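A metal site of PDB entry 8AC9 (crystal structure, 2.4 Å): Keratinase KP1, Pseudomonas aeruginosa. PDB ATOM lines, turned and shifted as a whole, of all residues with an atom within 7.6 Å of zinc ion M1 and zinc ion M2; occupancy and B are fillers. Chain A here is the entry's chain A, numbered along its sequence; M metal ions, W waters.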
ATOM      1  N   HIS A 270     -24.935   8.365  23.392  1.00  0.00           N
ATOM      2  CA  HIS A 270     -24.484   8.945  22.125  1.00  0.00           C
ATOM      3  C   HIS A 270     -22.974   9.177  22.150  1.00  0.00           C
ATOM      4  O   HIS A 270     -22.385   9.541  23.177  1.00  0.00           O
ATOM      5  CB  HIS A 270     -25.258  10.233  21.781  1.00  0.00           C
ATOM      6  CG  HIS A 270     -24.890  11.450  22.574  1.00  0.00           C
ATOM      7  ND1 HIS A 270     -23.883  12.314  22.204  1.00  0.00           N
ATOM      8  CD2 HIS A 270     -25.472  12.011  23.663  1.00  0.00           C
ATOM      9  CE1 HIS A 270     -23.824  13.318  23.062  1.00  0.00           C
ATOM     10  NE2 HIS A 270     -24.780  13.164  23.953  1.00  0.00           N
ATOM     11  N   ASP A 272     -21.223  10.950  19.610  1.00  0.00           N
ATOM     12  CA  ASP A 272     -20.779  12.184  18.956  1.00  0.00           C
ATOM     13  C   ASP A 272     -20.666  13.325  19.965  1.00  0.00           C
ATOM     14  O   ASP A 272     -21.330  13.328  21.013  1.00  0.00           O
ATOM     15  CB  ASP A 272     -21.719  12.608  17.829  1.00  0.00           C
ATOM     16  CG  ASP A 272     -23.142  12.912  18.306  1.00  0.00           C
ATOM     17  OD1 ASP A 272     -23.685  12.112  19.108  1.00  0.00           O
ATOM     18  OD2 ASP A 272     -23.740  13.920  17.862  1.00  0.00           O
ATOM     19  N   SER A 273     -19.790  14.252  19.641  1.00  0.00           N
ATOM     20  CA  SER A 273     -19.650  15.513  20.337  1.00  0.00           C
ATOM     21  C   SER A 273     -20.235  16.614  19.456  1.00  0.00           C
ATOM     22  O   SER A 273     -20.492  16.394  18.280  1.00  0.00           O
ATOM     23  CB  SER A 273     -18.176  15.810  20.617  1.00  0.00           C
ATOM     24  OG  SER A 273     -17.513  15.937  19.364  1.00  0.00           O
ATOM     25  N   VAL A 274     -20.385  17.815  20.019  1.00  0.00           N
ATOM     26  CA  VAL A 274     -20.655  19.000  19.196  1.00  0.00           C
ATOM     27  C   VAL A 274     -19.394  19.309  18.396  1.00  0.00           C
ATOM     28  O   VAL A 274     -18.321  18.738  18.647  1.00  0.00           O
ATOM     29  CB  VAL A 274     -21.070  20.230  20.020  1.00  0.00           C
ATOM     30  CG1 VAL A 274     -22.464  20.047  20.637  1.00  0.00           C
ATOM     31  CG2 VAL A 274     -20.034  20.515  21.071  1.00  0.00           C
ATOM     32  N   ASN A 281     -17.160  14.953  28.681  1.00  0.00           N
ATOM     33  CA  ASN A 281     -18.335  14.718  29.531  1.00  0.00           C
ATOM     34  C   ASN A 281     -19.566  14.445  28.676  1.00  0.00           C
ATOM     35  O   ASN A 281     -20.335  13.522  28.964  1.00  0.00           O
ATOM     36  CB  ASN A 281     -18.645  15.871  30.503  1.00  0.00           C
ATOM     37  CG  ASN A 281     -19.751  15.466  31.522  1.00  0.00           C
ATOM     38  OD1 ASN A 281     -19.768  14.321  31.986  1.00  0.00           O
ATOM     39  ND2 ASN A 281     -20.701  16.384  31.809  1.00  0.00           N
ATOM     40  N   ASP A 282     -19.761  15.262  27.643  1.00  0.00           N
ATOM     41  CA  ASP A 282     -20.914  15.154  26.746  1.00  0.00           C
ATOM     42  C   ASP A 282     -20.465  14.719  25.342  1.00  0.00           C
ATOM     43  O   ASP A 282     -20.139  15.561  24.508  1.00  0.00           O
ATOM     44  CB  ASP A 282     -21.656  16.488  26.711  1.00  0.00           C
ATOM     45  CG  ASP A 282     -22.902  16.417  25.896  1.00  0.00           C
ATOM     46  OD1 ASP A 282     -23.406  15.307  25.688  1.00  0.00           O
ATOM     47  OD2 ASP A 282     -23.369  17.473  25.433  1.00  0.00           O
ATOM     48  N   ASN A 283     -20.504  13.409  25.067  1.00  0.00           N
ATOM     49  CA  ASN A 283     -20.940  12.386  26.015  1.00  0.00           C
ATOM     50  C   ASN A 283     -19.961  11.224  26.015  1.00  0.00           C
ATOM     51  O   ASN A 283     -20.368  10.048  25.968  1.00  0.00           O
ATOM     52  CB  ASN A 283     -22.364  11.883  25.701  1.00  0.00           C
ATOM     53  CG  ASN A 283     -22.859  10.826  26.712  1.00  0.00           C
ATOM     54  OD1 ASN A 283     -22.609  10.941  27.918  1.00  0.00           O
ATOM     55  ND2 ASN A 283     -23.533   9.792  26.211  1.00  0.00           N
ATOM     56  N   GLY A 284     -18.688  11.533  26.058  1.00  0.00           N
ATOM     57  CA  GLY A 284     -17.712  10.486  26.312  1.00  0.00           C
ATOM     58  C   GLY A 284     -18.017   9.721  27.580  1.00  0.00           C
ATOM     59  O   GLY A 284     -17.806   8.509  27.656  1.00  0.00           O
ATOM     60  N   GLU A 314     -26.368  12.727  17.718  1.00  0.00           N
ATOM     61  CA  GLU A 314     -27.332  13.167  18.710  1.00  0.00           C
ATOM     62  C   GLU A 314     -27.352  14.685  18.812  1.00  0.00           C
ATOM     63  O   GLU A 314     -28.401  15.279  19.060  1.00  0.00           O
ATOM     64  CB  GLU A 314     -27.005  12.569  20.072  1.00  0.00           C
ATOM     65  CG  GLU A 314     -28.003  12.949  21.156  1.00  0.00           C
ATOM     66  CD  GLU A 314     -27.592  14.152  21.944  1.00  0.00           C
ATOM     67  OE1 GLU A 314     -26.462  14.658  21.704  1.00  0.00           O
ATOM     68  OE2 GLU A 314     -28.399  14.595  22.796  1.00  0.00           O
ATOM     69  N   GLU A 315     -26.196  15.304  18.687  1.00  0.00           N
ATOM     70  CA  GLU A 315     -26.083  16.747  18.812  1.00  0.00           C
ATOM     71  C   GLU A 315     -26.712  17.476  17.617  1.00  0.00           C
ATOM     72  O   GLU A 315     -26.925  18.679  17.705  1.00  0.00           O
ATOM     73  CB  GLU A 315     -24.615  17.140  18.956  1.00  0.00           C
ATOM     74  CG  GLU A 315     -23.890  16.446  20.108  1.00  0.00           C
ATOM     75  CD  GLU A 315     -24.287  17.003  21.476  1.00  0.00           C
ATOM     76  OE1 GLU A 315     -25.341  17.645  21.571  1.00  0.00           O
ATOM     77  OE2 GLU A 315     -23.544  16.806  22.445  1.00  0.00           O
ATOM     78  N   ASN A 341     -30.723   5.150  29.228  1.00  0.00           N
ATOM     79  CA  ASN A 341     -29.959   6.184  28.535  1.00  0.00           C
ATOM     80  C   ASN A 341     -28.920   6.785  29.463  1.00  0.00           C
ATOM     81  O   ASN A 341     -29.232   7.117  30.618  1.00  0.00           O
ATOM     82  CB  ASN A 341     -30.892   7.271  27.996  1.00  0.00           C
ATOM     83  CG  ASN A 341     -30.198   8.167  27.036  1.00  0.00           C
ATOM     84  OD1 ASN A 341     -29.729   7.733  25.990  1.00  0.00           O
ATOM     85  ND2 ASN A 341     -30.111   9.441  27.385  1.00  0.00           N
ATOM     86  N   PHE A 342     -27.696   6.935  28.979  1.00  0.00           N
ATOM     87  CA  PHE A 342     -26.624   7.515  29.786  1.00  0.00           C
ATOM     88  C   PHE A 342     -25.954   8.634  29.000  1.00  0.00           C
ATOM     89  O   PHE A 342     -25.101   8.386  28.136  1.00  0.00           O
ATOM     90  CB  PHE A 342     -25.649   6.434  30.219  1.00  0.00           C
ATOM     91  CG  PHE A 342     -26.313   5.323  30.951  1.00  0.00           C
ATOM     92  CD1 PHE A 342     -26.714   5.508  32.268  1.00  0.00           C
ATOM     93  CD2 PHE A 342     -26.654   4.153  30.298  1.00  0.00           C
ATOM     94  CE1 PHE A 342     -27.393   4.516  32.939  1.00  0.00           C
ATOM     95  CE2 PHE A 342     -27.324   3.167  30.952  1.00  0.00           C
ATOM     96  CZ  PHE A 342     -27.697   3.338  32.279  1.00  0.00           C
ATOM     97  N   ASP A 343     -26.327   9.867  29.322  1.00  0.00           N
ATOM     98  CA  ASP A 343     -25.882  11.054  28.592  1.00  0.00           C
ATOM     99  C   ASP A 343     -25.448  12.111  29.603  1.00  0.00           C
ATOM    100  O   ASP A 343     -26.290  12.761  30.224  1.00  0.00           O
ATOM    101  CB  ASP A 343     -27.002  11.572  27.675  1.00  0.00           C
ATOM    102  CG  ASP A 343     -26.541  12.703  26.756  1.00  0.00           C
ATOM    103  OD1 ASP A 343     -25.402  13.209  26.927  1.00  0.00           O
ATOM    104  OD2 ASP A 343     -27.323  13.079  25.841  1.00  0.00           O
ATOM    105  N   MET A 344     -24.140  12.286  29.748  1.00  0.00           N
ATOM    106  CA  MET A 344     -23.550  13.229  30.696  1.00  0.00           C
ATOM    107  C   MET A 344     -23.683  12.699  32.118  1.00  0.00           C
ATOM    108  O   MET A 344     -24.715  12.916  32.778  1.00  0.00           O
ATOM    109  CB  MET A 344     -24.161  14.634  30.554  1.00  0.00           C
ATOM    110  CG  MET A 344     -24.052  15.274  29.146  1.00  0.00           C
ATOM    111  SD  MET A 344     -24.552  17.035  29.122  1.00  0.00           S
ATOM    112  CE  MET A 344     -23.343  17.747  30.253  1.00  0.00           C
ATOM    113  N   ARG A 396     -34.278  15.834  25.423  1.00  0.00           N
ATOM    114  CA  ARG A 396     -33.025  16.362  24.900  1.00  0.00           C
ATOM    115  C   ARG A 396     -31.959  15.287  24.740  1.00  0.00           C
ATOM    116  O   ARG A 396     -30.776  15.623  24.611  1.00  0.00           O
ATOM    117  CB  ARG A 396     -32.494  17.507  25.780  1.00  0.00           C
ATOM    118  CG  ARG A 396     -32.965  18.890  25.337  1.00  0.00           C
ATOM    119  CD  ARG A 396     -32.765  19.950  26.424  1.00  0.00           C
ATOM    120  NE  ARG A 396     -31.361  20.356  26.537  1.00  0.00           N
ATOM    121  CZ  ARG A 396     -30.896  21.150  27.494  1.00  0.00           C
ATOM    122  NH1 ARG A 396     -31.717  21.639  28.415  1.00  0.00           N
ATOM    123  NH2 ARG A 396     -29.608  21.472  27.526  1.00  0.00           N
ATOM    124  N   SER A 397     -32.359  14.018  24.712  1.00  0.00           N
ATOM    125  CA  SER A 397     -31.408  12.945  24.453  1.00  0.00           C
ATOM    126  C   SER A 397     -32.135  11.787  23.784  1.00  0.00           C
ATOM    127  O   SER A 397     -33.319  11.877  23.443  1.00  0.00           O
ATOM    128  CB  SER A 397     -30.724  12.493  25.753  1.00  0.00           C
ATOM    129  OG  SER A 397     -29.468  11.879  25.479  1.00  0.00           O
ATOM    130  N   ASP A 398     -31.437  10.652  23.664  1.00  0.00           N
ATOM    131  CA  ASP A 398     -31.766   9.606  22.726  1.00  0.00           C
ATOM    132  C   ASP A 398     -32.890   8.684  23.191  1.00  0.00           C
ATOM    133  O   ASP A 398     -33.324   7.819  22.428  1.00  0.00           O
ATOM    134  CB  ASP A 398     -30.509   8.807  22.423  1.00  0.00           C
ATOM    135  CG  ASP A 398     -29.497   9.624  21.632  1.00  0.00           C
ATOM    136  OD1 ASP A 398     -29.791   9.978  20.475  1.00  0.00           O
ATOM    137  OD2 ASP A 398     -28.430   9.933  22.184  1.00  0.00           O
ATOM    138  N   PHE A 413     -28.176  11.360  34.760  1.00  0.00           N
ATOM    139  CA  PHE A 413     -27.772  12.658  34.251  1.00  0.00           C
ATOM    140  C   PHE A 413     -27.113  13.396  35.414  1.00  0.00           C
ATOM    141  O   PHE A 413     -27.622  13.330  36.534  1.00  0.00           O
ATOM    142  CB  PHE A 413     -29.002  13.396  33.711  1.00  0.00           C
ATOM    143  CG  PHE A 413     -28.740  14.786  33.169  1.00  0.00           C
ATOM    144  CD1 PHE A 413     -27.666  15.037  32.341  1.00  0.00           C
ATOM    145  CD2 PHE A 413     -29.612  15.836  33.475  1.00  0.00           C
ATOM    146  CE1 PHE A 413     -27.450  16.325  31.822  1.00  0.00           C
ATOM    147  CE2 PHE A 413     -29.417  17.118  32.965  1.00  0.00           C
ATOM    148  CZ  PHE A 413     -28.348  17.362  32.132  1.00  0.00           C
ATOM    149  N   ALA A 416     -26.283  19.818  33.031  1.00  0.00           N
ATOM    150  CA  ALA A 416     -25.612  20.514  31.951  1.00  0.00           C
ATOM    151  C   ALA A 416     -25.508  22.003  32.254  1.00  0.00           C
ATOM    152  O   ALA A 416     -24.770  22.398  33.171  1.00  0.00           O
ATOM    153  CB  ALA A 416     -26.325  20.262  30.634  1.00  0.00           C
ATOM    154  N   TYR A 440     -20.127  22.862  29.186  1.00  0.00           N
ATOM    155  CA  TYR A 440     -21.115  22.294  28.299  1.00  0.00           C
ATOM    156  C   TYR A 440     -20.920  22.765  26.853  1.00  0.00           C
ATOM    157  O   TYR A 440     -20.895  23.960  26.566  1.00  0.00           O
ATOM    158  CB  TYR A 440     -22.496  22.686  28.830  1.00  0.00           C
ATOM    159  CG  TYR A 440     -23.625  22.137  28.039  1.00  0.00           C
ATOM    160  CD1 TYR A 440     -23.757  20.758  27.831  1.00  0.00           C
ATOM    161  CD2 TYR A 440     -24.570  22.983  27.479  1.00  0.00           C
ATOM    162  CE1 TYR A 440     -24.816  20.236  27.089  1.00  0.00           C
ATOM    163  CE2 TYR A 440     -25.639  22.478  26.725  1.00  0.00           C
ATOM    164  CZ  TYR A 440     -25.753  21.110  26.542  1.00  0.00           C
ATOM    165  OH  TYR A 440     -26.790  20.598  25.803  1.00  0.00           O
ATOM    166  N   HIS A 441     -20.770  21.810  25.936  1.00  0.00           N
ATOM    167  CA  HIS A 441     -20.718  22.100  24.503  1.00  0.00           C
ATOM    168  C   HIS A 441     -19.575  23.043  24.164  1.00  0.00           C
ATOM    169  O   HIS A 441     -19.672  23.821  23.218  1.00  0.00           O
ATOM    170  CB  HIS A 441     -22.054  22.661  24.009  1.00  0.00           C
ATOM    171  CG  HIS A 441     -23.110  21.613  23.808  1.00  0.00           C
ATOM    172  ND1 HIS A 441     -24.297  21.850  23.147  1.00  0.00           N
ATOM    173  CD2 HIS A 441     -23.148  20.305  24.178  1.00  0.00           C
ATOM    174  CE1 HIS A 441     -25.020  20.739  23.118  1.00  0.00           C
ATOM    175  NE2 HIS A 441     -24.339  19.784  23.735  1.00  0.00           N
ATOM    176  N   ASP A 445     -14.580  21.010  27.256  1.00  0.00           N
ATOM    177  CA  ASP A 445     -15.208  19.760  27.732  1.00  0.00           C
ATOM    178  C   ASP A 445     -14.263  18.599  27.439  1.00  0.00           C
ATOM    179  O   ASP A 445     -14.517  17.719  26.614  1.00  0.00           O
ATOM    180  CB  ASP A 445     -16.582  19.533  27.090  1.00  0.00           C
ATOM    181  CG  ASP A 445     -17.259  18.231  27.567  1.00  0.00           C
ATOM    182  OD1 ASP A 445     -16.773  17.645  28.567  1.00  0.00           O
ATOM    183  OD2 ASP A 445     -18.257  17.785  26.933  1.00  0.00           O
HETATM  184 ZN    ZN M   1     -24.906  17.665  23.955  1.00  0.00          ZN
HETATM  185 ZN    ZN M   2     -25.281  14.582  25.286  1.00  0.00          ZN
HETATM  186  O   HOH W   1     -26.214  15.998  23.790  1.00  0.00           O
HETATM  187  O   HOH W   2     -27.000  18.065  24.948  1.00  0.00           O
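CB of Asn 283 touches zinc ion M2, 3.996 Å away. Glu 314 touches zinc ion M2. Five residues have an atom within 4 Å of zinc ion M2: His 270, Asp 282, Asn 283, Glu 314 and Asp 343.
OH of Tyr 440 touches zinc ion M1 (3.9 Å). Four residues have an atom within 4 Å of zinc ion M1: Asp 282, Glu 315, Tyr 440 and His 441.
NE2 of His 270 sits close to OE1 of Glu 314 (3.2 Å). The side-chain amide nitrogen (ND2) of Asn 283 is in hydrogen-bond range of the backbone carbonyl oxygen (O) of Phe 342, 2.9 Å away. The backbone NH of Asp 282 lies within hydrogen-bond range of the side-chain carboxylate of Asp 445 (3.0 Å). OH of Tyr 440 is in hydrogen-bond range of NH2 of Arg 396 (3.4 Å). OD2 of Asp 272 sits at hydrogen-bond distance from N of Glu 314 (2.9 Å). The side-chain hydroxyl (OH) of Tyr 440 lies close to a ring nitrogen (NE2) of His 441 (3.3 Å). OG of Ser 397 lies close to OD2 of Asp 343, 2.5 Å away. N of Glu 315 sits at hydrogen-bond distance from OD2 of Asp 272 (2.9 Å).
Zinc ion M2 is bound by NE2 of His 270 (2.0 Å), OD1 of Asp 282 (2.1 Å), OD1 of Asp 343 (2.1 Å), water W1 (2.3 Å) and OD2 of Asp 343 (2.6 Å). Zinc ion M2 has five donor atoms within binding distance.
Water W1 is bound to zinc ion M1, 2.1 Å away. Zinc ion M1 is bound by OD2 of Asp 282 (2.1 Å). NE2 of His 441 is bound to zinc ion M1 (2.2 Å). Zinc ion M1 is bound by the side-chain carboxylate (OE2) of Glu 315 (2.2 Å). Zinc ion M1 is bound by water W2. Zinc ion M1 is bound by the side-chain carboxylate (OE1) of Glu 315 (2.4 Å). Zinc ion M1 has six donor atoms within binding distance.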
